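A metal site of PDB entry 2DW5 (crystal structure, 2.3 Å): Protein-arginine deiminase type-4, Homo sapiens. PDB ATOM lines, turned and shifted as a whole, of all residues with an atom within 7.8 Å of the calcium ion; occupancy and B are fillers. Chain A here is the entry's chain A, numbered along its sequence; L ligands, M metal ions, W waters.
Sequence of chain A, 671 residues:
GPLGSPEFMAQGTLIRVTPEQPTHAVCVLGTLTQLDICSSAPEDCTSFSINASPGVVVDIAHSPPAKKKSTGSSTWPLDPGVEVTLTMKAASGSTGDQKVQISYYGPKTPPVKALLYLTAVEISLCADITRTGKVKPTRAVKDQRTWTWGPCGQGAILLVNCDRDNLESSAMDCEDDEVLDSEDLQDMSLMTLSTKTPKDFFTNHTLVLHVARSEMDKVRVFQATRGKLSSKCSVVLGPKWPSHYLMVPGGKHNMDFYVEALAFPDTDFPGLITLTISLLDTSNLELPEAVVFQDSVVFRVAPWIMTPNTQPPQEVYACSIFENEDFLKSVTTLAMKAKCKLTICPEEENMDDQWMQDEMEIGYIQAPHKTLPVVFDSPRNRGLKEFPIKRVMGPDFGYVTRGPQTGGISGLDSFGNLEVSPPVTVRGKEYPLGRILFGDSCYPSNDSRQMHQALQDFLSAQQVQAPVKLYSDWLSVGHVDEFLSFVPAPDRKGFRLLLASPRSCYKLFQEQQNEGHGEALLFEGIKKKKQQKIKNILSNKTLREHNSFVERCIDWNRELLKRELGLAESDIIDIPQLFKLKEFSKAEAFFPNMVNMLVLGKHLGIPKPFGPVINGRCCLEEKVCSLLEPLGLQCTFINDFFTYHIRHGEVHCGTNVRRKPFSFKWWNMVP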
ATOM      1  N   MET A 306      23.431 -28.231  25.225  1.00  0.00           N
ATOM      2  CA  MET A 306      23.310 -28.239  23.771  1.00  0.00           C
ATOM      3  C   MET A 306      24.426 -29.066  23.167  1.00  0.00           C
ATOM      4  O   MET A 306      25.446 -29.319  23.820  1.00  0.00           O
ATOM      5  CB  MET A 306      23.418 -26.826  23.207  1.00  0.00           C
ATOM      6  CG  MET A 306      22.193 -25.990  23.467  1.00  0.00           C
ATOM      7  SD  MET A 306      22.440 -24.310  22.850  1.00  0.00           S
ATOM      8  CE  MET A 306      22.495 -24.720  21.064  1.00  0.00           C
ATOM      9  N   ASN A 309      27.596 -28.693  16.115  1.00  0.00           N
ATOM     10  CA  ASN A 309      27.525 -29.321  14.801  1.00  0.00           C
ATOM     11  C   ASN A 309      28.562 -30.404  14.610  1.00  0.00           C
ATOM     12  O   ASN A 309      28.522 -31.135  13.608  1.00  0.00           O
ATOM     13  CB  ASN A 309      27.815 -28.277  13.741  1.00  0.00           C
ATOM     14  CG  ASN A 309      26.701 -27.299  13.566  1.00  0.00           C
ATOM     15  OD1 ASN A 309      25.585 -27.469  14.097  1.00  0.00           O
ATOM     16  ND2 ASN A 309      26.959 -26.273  12.759  1.00  0.00           N
ATOM     17  N   MET A 356      11.984 -24.377  10.764  1.00  0.00           N
ATOM     18  CA  MET A 356      12.137 -25.475  11.747  1.00  0.00           C
ATOM     19  C   MET A 356      13.407 -25.299  12.652  1.00  0.00           C
ATOM     20  O   MET A 356      13.489 -25.895  13.746  1.00  0.00           O
ATOM     21  CB  MET A 356      12.152 -26.805  10.991  1.00  0.00           C
ATOM     22  CG  MET A 356      12.415 -28.048  11.812  1.00  0.00           C
ATOM     23  SD  MET A 356      11.156 -28.451  13.034  1.00  0.00           S
ATOM     24  CE  MET A 356       9.869 -29.272  12.051  1.00  0.00           C
ATOM     25  N   GLN A 357      14.341 -24.476  12.216  1.00  0.00           N
ATOM     26  CA  GLN A 357      15.466 -24.065  13.070  1.00  0.00           C
ATOM     27  C   GLN A 357      15.050 -23.239  14.295  1.00  0.00           C
ATOM     28  O   GLN A 357      15.743 -23.228  15.321  1.00  0.00           O
ATOM     29  CB  GLN A 357      16.446 -23.227  12.254  1.00  0.00           C
ATOM     30  CG  GLN A 357      17.636 -22.622  13.043  1.00  0.00           C
ATOM     31  CD  GLN A 357      18.604 -23.687  13.563  1.00  0.00           C
ATOM     32  OE1 GLN A 357      19.255 -23.473  14.564  1.00  0.00           O
ATOM     33  NE2 GLN A 357      18.673 -24.842  12.891  1.00  0.00           N
ATOM     34  N   ASP A 358      13.943 -22.528  14.186  1.00  0.00           N
ATOM     35  CA  ASP A 358      13.722 -21.364  15.021  1.00  0.00           C
ATOM     36  C   ASP A 358      12.817 -21.527  16.262  1.00  0.00           C
ATOM     37  O   ASP A 358      12.995 -20.771  17.227  1.00  0.00           O
ATOM     38  CB  ASP A 358      13.239 -20.226  14.105  1.00  0.00           C
ATOM     39  CG  ASP A 358      14.354 -19.666  13.197  1.00  0.00           C
ATOM     40  OD1 ASP A 358      15.569 -19.802  13.524  1.00  0.00           O
ATOM     41  OD2 ASP A 358      14.006 -19.056  12.169  1.00  0.00           O
ATOM     42  N   MET A 360      12.705 -24.276  18.122  1.00  0.00           N
ATOM     43  CA  MET A 360      13.223 -25.255  19.072  1.00  0.00           C
ATOM     44  C   MET A 360      14.728 -25.532  18.941  1.00  0.00           C
ATOM     45  O   MET A 360      15.331 -25.328  17.890  1.00  0.00           O
ATOM     46  CB  MET A 360      12.440 -26.540  18.941  1.00  0.00           C
ATOM     47  CG  MET A 360      12.898 -27.401  17.813  1.00  0.00           C
ATOM     48  SD  MET A 360      11.926 -28.903  17.665  1.00  0.00           S
ATOM     49  CE  MET A 360      13.010 -29.864  16.586  1.00  0.00           C
ATOM     50  N   GLU A 361      15.286 -26.042  20.043  1.00  0.00           N
ATOM     51  CA  GLU A 361      16.678 -26.485  20.113  1.00  0.00           C
ATOM     52  C   GLU A 361      16.725 -27.802  20.880  1.00  0.00           C
ATOM     53  O   GLU A 361      16.155 -27.920  21.967  1.00  0.00           O
ATOM     54  CB  GLU A 361      17.536 -25.418  20.805  1.00  0.00           C
ATOM     55  CG  GLU A 361      19.015 -25.716  20.857  1.00  0.00           C
ATOM     56  CD  GLU A 361      19.756 -25.452  19.562  1.00  0.00           C
ATOM     57  OE1 GLU A 361      19.519 -24.401  18.942  1.00  0.00           O
ATOM     58  OE2 GLU A 361      20.616 -26.290  19.175  1.00  0.00           O
ATOM     59  N   ILE A 362      17.364 -28.818  20.286  1.00  0.00           N
ATOM     60  CA  ILE A 362      17.347 -30.154  20.899  1.00  0.00           C
ATOM     61  C   ILE A 362      18.660 -30.325  21.599  1.00  0.00           C
ATOM     62  O   ILE A 362      19.703 -30.392  20.976  1.00  0.00           O
ATOM     63  CB  ILE A 362      17.131 -31.327  19.902  1.00  0.00           C
ATOM     64  CG1 ILE A 362      15.975 -31.042  18.943  1.00  0.00           C
ATOM     65  CG2 ILE A 362      16.901 -32.665  20.643  1.00  0.00           C
ATOM     66  CD1 ILE A 362      14.616 -31.242  19.509  1.00  0.00           C
ATOM     67  N   SER A 414      14.445 -16.394  18.375  1.00  0.00           N
ATOM     68  CA  SER A 414      14.406 -17.562  17.494  1.00  0.00           C
ATOM     69  C   SER A 414      15.736 -18.302  17.604  1.00  0.00           C
ATOM     70  O   SER A 414      16.809 -17.695  17.729  1.00  0.00           O
ATOM     71  CB  SER A 414      14.100 -17.174  16.037  1.00  0.00           C
ATOM     72  OG  SER A 414      12.832 -16.503  15.943  1.00  0.00           O
ATOM     73  N   PHE A 415      15.665 -19.625  17.586  1.00  0.00           N
ATOM     74  CA  PHE A 415      16.790 -20.443  18.013  1.00  0.00           C
ATOM     75  C   PHE A 415      17.769 -20.714  16.921  1.00  0.00           C
ATOM     76  O   PHE A 415      18.733 -21.411  17.130  1.00  0.00           O
ATOM     77  CB  PHE A 415      16.302 -21.717  18.699  1.00  0.00           C
ATOM     78  CG  PHE A 415      15.798 -21.491  20.128  1.00  0.00           C
ATOM     79  CD1 PHE A 415      15.279 -22.542  20.854  1.00  0.00           C
ATOM     80  CD2 PHE A 415      15.832 -20.228  20.728  1.00  0.00           C
ATOM     81  CE1 PHE A 415      14.825 -22.376  22.148  1.00  0.00           C
ATOM     82  CE2 PHE A 415      15.364 -20.036  22.027  1.00  0.00           C
ATOM     83  CZ  PHE A 415      14.877 -21.126  22.729  1.00  0.00           C
ATOM     84  N   GLY A 416      17.570 -20.070  15.772  1.00  0.00           N
ATOM     85  CA  GLY A 416      18.658 -19.819  14.837  1.00  0.00           C
ATOM     86  C   GLY A 416      19.653 -18.853  15.432  1.00  0.00           C
ATOM     87  O   GLY A 416      20.816 -18.808  14.987  1.00  0.00           O
ATOM     88  N   ASN A 417      19.203 -18.077  16.429  1.00  0.00           N
ATOM     89  CA  ASN A 417      20.093 -17.219  17.209  1.00  0.00           C
ATOM     90  C   ASN A 417      20.685 -17.923  18.441  1.00  0.00           C
ATOM     91  O   ASN A 417      21.320 -17.269  19.262  1.00  0.00           O
ATOM     92  CB  ASN A 417      19.392 -15.905  17.659  1.00  0.00           C
ATOM     93  CG  ASN A 417      20.397 -14.825  18.081  1.00  0.00           C
ATOM     94  OD1 ASN A 417      21.495 -14.731  17.500  1.00  0.00           O
ATOM     95  ND2 ASN A 417      20.075 -14.064  19.126  1.00  0.00           N
ATOM     96  N   LEU A 418      20.453 -19.241  18.564  1.00  0.00           N
ATOM     97  CA  LEU A 418      21.066 -20.034  19.637  1.00  0.00           C
ATOM     98  C   LEU A 418      21.925 -21.146  19.068  1.00  0.00           C
ATOM     99  O   LEU A 418      21.403 -22.033  18.402  1.00  0.00           O
ATOM    100  CB  LEU A 418      19.935 -20.633  20.488  1.00  0.00           C
ATOM    101  CG  LEU A 418      20.197 -21.437  21.770  1.00  0.00           C
ATOM    102  CD1 LEU A 418      21.008 -20.687  22.689  1.00  0.00           C
ATOM    103  CD2 LEU A 418      18.861 -21.754  22.378  1.00  0.00           C
ATOM    104  N   GLU A 419      23.233 -21.074  19.312  1.00  0.00           N
ATOM    105  CA  GLU A 419      24.234 -22.095  18.852  1.00  0.00           C
ATOM    106  C   GLU A 419      25.205 -22.441  19.995  1.00  0.00           C
ATOM    107  O   GLU A 419      25.107 -21.801  21.058  1.00  0.00           O
ATOM    108  CB  GLU A 419      24.976 -21.557  17.640  1.00  0.00           C
ATOM    109  CG  GLU A 419      24.039 -21.155  16.435  1.00  0.00           C
ATOM    110  CD  GLU A 419      23.255 -22.340  15.803  1.00  0.00           C
ATOM    111  OE1 GLU A 419      22.042 -22.197  15.469  1.00  0.00           O
ATOM    112  OE2 GLU A 419      23.866 -23.426  15.671  1.00  0.00           O
ATOM    113  N   VAL A 420      26.072 -23.465  19.807  1.00  0.00           N
ATOM    114  CA  VAL A 420      27.212 -23.811  20.745  1.00  0.00           C
ATOM    115  C   VAL A 420      28.491 -24.091  19.960  1.00  0.00           C
ATOM    116  O   VAL A 420      28.457 -24.721  18.884  1.00  0.00           O
ATOM    117  CB  VAL A 420      27.169 -25.280  21.424  1.00  0.00           C
ATOM    118  CG1 VAL A 420      27.556 -25.278  22.932  1.00  0.00           C
ATOM    119  CG2 VAL A 420      25.891 -26.063  21.058  1.00  0.00           C
ATOM    120  N   LEU A 437      26.654 -19.897  22.278  1.00  0.00           N
ATOM    121  CA  LEU A 437      26.890 -18.695  21.485  1.00  0.00           C
ATOM    122  C   LEU A 437      25.459 -18.161  21.159  1.00  0.00           C
ATOM    123  O   LEU A 437      24.624 -18.916  20.650  1.00  0.00           O
ATOM    124  CB  LEU A 437      27.580 -19.132  20.173  1.00  0.00           C
ATOM    125  CG  LEU A 437      29.115 -19.123  19.978  1.00  0.00           C
ATOM    126  CD1 LEU A 437      29.906 -18.883  21.226  1.00  0.00           C
ATOM    127  CD2 LEU A 437      29.622 -20.301  19.072  1.00  0.00           C
ATOM    128  N   VAL A 480      22.871 -15.611  14.784  1.00  0.00           N
ATOM    129  CA  VAL A 480      24.300 -15.932  14.654  1.00  0.00           C
ATOM    130  C   VAL A 480      24.533 -16.954  13.517  1.00  0.00           C
ATOM    131  O   VAL A 480      25.608 -16.993  12.960  1.00  0.00           O
ATOM    132  CB  VAL A 480      24.998 -16.387  15.987  1.00  0.00           C
ATOM    133  CG1 VAL A 480      25.076 -15.201  17.042  1.00  0.00           C
ATOM    134  CG2 VAL A 480      24.368 -17.649  16.560  1.00  0.00           C
ATOM    135  N   ASP A 481      23.533 -17.747  13.164  1.00  0.00           N
ATOM    136  CA  ASP A 481      23.683 -18.773  12.105  1.00  0.00           C
ATOM    137  C   ASP A 481      23.754 -18.114  10.732  1.00  0.00           C
ATOM    138  O   ASP A 481      24.223 -18.697   9.794  1.00  0.00           O
ATOM    139  CB  ASP A 481      22.654 -19.946  12.238  1.00  0.00           C
ATOM    140  CG  ASP A 481      21.192 -19.581  11.816  1.00  0.00           C
ATOM    141  OD1 ASP A 481      20.369 -20.559  11.642  1.00  0.00           O
ATOM    142  OD2 ASP A 481      20.838 -18.367  11.669  1.00  0.00           O
ATOM    143  N   HIS A 652      19.904 -24.152   6.802  1.00  0.00           N
ATOM    144  CA  HIS A 652      19.994 -24.283   8.258  1.00  0.00           C
ATOM    145  C   HIS A 652      18.713 -23.752   8.878  1.00  0.00           C
ATOM    146  O   HIS A 652      18.114 -24.394   9.738  1.00  0.00           O
ATOM    147  CB  HIS A 652      21.209 -23.509   8.803  1.00  0.00           C
ATOM    148  CG  HIS A 652      21.594 -23.862  10.209  1.00  0.00           C
ATOM    149  ND1 HIS A 652      21.187 -23.120  11.303  1.00  0.00           N
ATOM    150  CD2 HIS A 652      22.339 -24.874  10.706  1.00  0.00           C
ATOM    151  CE1 HIS A 652      21.675 -23.653  12.413  1.00  0.00           C
ATOM    152  NE2 HIS A 652      22.373 -24.730  12.083  1.00  0.00           N
ATOM    153  N   THR A 655      15.835 -26.237   8.758  1.00  0.00           N
ATOM    154  CA  THR A 655      16.075 -27.570   9.346  1.00  0.00           C
ATOM    155  C   THR A 655      16.501 -27.550  10.828  1.00  0.00           C
ATOM    156  O   THR A 655      16.850 -26.508  11.388  1.00  0.00           O
ATOM    157  CB  THR A 655      17.157 -28.373   8.538  1.00  0.00           C
ATOM    158  OG1 THR A 655      18.411 -27.681   8.585  1.00  0.00           O
ATOM    159  CG2 THR A 655      16.730 -28.607   7.055  1.00  0.00           C
ATOM    160  N   ASN A 656      16.456 -28.730  11.461  1.00  0.00           N
ATOM    161  CA  ASN A 656      16.989 -28.891  12.818  1.00  0.00           C
ATOM    162  C   ASN A 656      17.534 -30.325  13.005  1.00  0.00           C
ATOM    163  O   ASN A 656      17.152 -31.226  12.267  1.00  0.00           O
ATOM    164  CB  ASN A 656      15.928 -28.514  13.891  1.00  0.00           C
ATOM    165  CG  ASN A 656      16.534 -27.767  15.054  1.00  0.00           C
ATOM    166  OD1 ASN A 656      17.626 -28.124  15.526  1.00  0.00           O
ATOM    167  ND2 ASN A 656      15.863 -26.698  15.514  1.00  0.00           N
ATOM    168  N   ARG A 659      21.561 -34.463  17.917  1.00  0.00           N
ATOM    169  CA  ARG A 659      22.903 -34.972  17.778  1.00  0.00           C
ATOM    170  C   ARG A 659      23.263 -35.702  19.039  1.00  0.00           C
ATOM    171  O   ARG A 659      22.603 -35.542  20.079  1.00  0.00           O
ATOM    172  CB  ARG A 659      23.895 -33.832  17.600  1.00  0.00           C
ATOM    173  CG  ARG A 659      23.610 -33.014  16.379  1.00  0.00           C
ATOM    174  CD  ARG A 659      24.610 -31.936  16.146  1.00  0.00           C
ATOM    175  NE  ARG A 659      24.662 -31.641  14.713  1.00  0.00           N
ATOM    176  CZ  ARG A 659      24.078 -30.611  14.138  1.00  0.00           C
ATOM    177  NH1 ARG A 659      23.401 -29.709  14.867  1.00  0.00           N
ATOM    178  NH2 ARG A 659      24.179 -30.456  12.835  1.00  0.00           N
HETATM  179  O1  LIG L   1      11.934 -15.275  11.074  1.00  0.00           O
HETATM  180  C1  LIG L   1      12.002 -14.770   9.983  1.00  0.00           C
HETATM  181  N1  LIG L   1      12.236 -13.468   9.791  1.00  0.00           N
HETATM  182  C2  LIG L   1      11.813 -15.672   8.809  1.00  0.00           C
HETATM  183  C3  LIG L   1      13.163 -16.038   8.197  1.00  0.00           C
HETATM  184  C4  LIG L   1      14.360 -16.092   9.131  1.00  0.00           C
HETATM  185  C5  LIG L   1      14.502 -17.334  10.005  1.00  0.00           C
HETATM  186  N2  LIG L   1      15.876 -17.721   9.709  1.00  0.00           N
HETATM  187  C6  LIG L   1      16.969 -18.307  10.210  1.00  0.00           C
HETATM  188  C7  LIG L   1      17.964 -18.222   9.087  1.00  0.00           C
HETATM  189  N3  LIG L   1      17.196 -18.923  11.368  1.00  0.00           N
HETATM  190  N4  LIG L   1      11.013 -15.089   7.711  1.00  0.00           N
HETATM  191  C8  LIG L   1       9.793 -14.557   7.860  1.00  0.00           C
HETATM  192  O2  LIG L   1       9.245 -14.526   8.951  1.00  0.00           O
HETATM  193  C9  LIG L   1       9.084 -13.987   6.657  1.00  0.00           C
HETATM  194  C10 LIG L   1       9.770 -13.735   5.456  1.00  0.00           C
HETATM  195  C11 LIG L   1       7.711 -13.683   6.707  1.00  0.00           C
HETATM  196  C12 LIG L   1       7.056 -13.151   5.589  1.00  0.00           C
HETATM  197  C13 LIG L   1       7.757 -12.911   4.411  1.00  0.00           C
HETATM  198  C14 LIG L   1       9.115 -13.203   4.337  1.00  0.00           C
HETATM  199 CA    CA M   1      20.073 -23.243  16.716  1.00  0.00          CA
HETATM  200  O   HOH W   1      21.419 -25.386  16.641  1.00  0.00           O
HETATM  201  O   HOH W   2      17.696 -24.151  16.548  1.00  0.00           O
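The calcium ion is bound by the backbone carbonyl oxygen (O) of Phe 415, 2.3 Å away. The calcium ion is bound by OE1 of Gln 357. The calcium ion is bound by O of Leu 418, 2.5 Å away. The calcium ion is bound by water W1, 2.5 Å away. Water W2 binds the calcium ion. The calcium ion is bound by OE1 of Glu 419 (2.6 Å). The calcium ion is bound by OE1 of Glu 361, at 2.6 Å. The calcium ion has seven donor atoms within binding distance.
Within 4 Å of the calcium ion: Gln 357, Glu 361, Phe 415, Leu 418 and Glu 419.
OD1 of Asp 358 lies within salt-bridge range of N3 of the ligand, 2.8 Å away. A nitrogen (N3) of the ligand is in salt-bridge range of the side-chain carboxylate (OD1) of Asp 481, 3.6 Å away.
O of Thr 655 lies within hydrogen-bond range of NE2 of Gln 357 (2.9 Å). The backbone carbonyl oxygen (O) of Glu 419 sits at hydrogen-bond distance from the backbone NH (N) of Leu 437. The side-chain amide nitrogen (NE2) of Gln 357 is in hydrogen-bond range of the backbone carbonyl oxygen (O) of His 652, at 3.2 Å. The backbone NH (N) of Phe 415 lies within hydrogen-bond range of the backbone carbonyl oxygen (O) of Asp 358 (2.9 Å). O of Gln 357 is in hydrogen-bond range of ND2 of Asn 656 (3.5 Å).
Water W2 lies within hydrogen-bond range of O of Gln 357 (2.5 Å), O of Met 360 (3.0 Å) and ND2 of Asn 656 (3.3 Å). Water W1 bridges the side-chain carboxylate (OE2) of Glu 361 (2.8 Å) and the side-chain carboxylate (OE2) of Glu 419 (3.3 Å).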
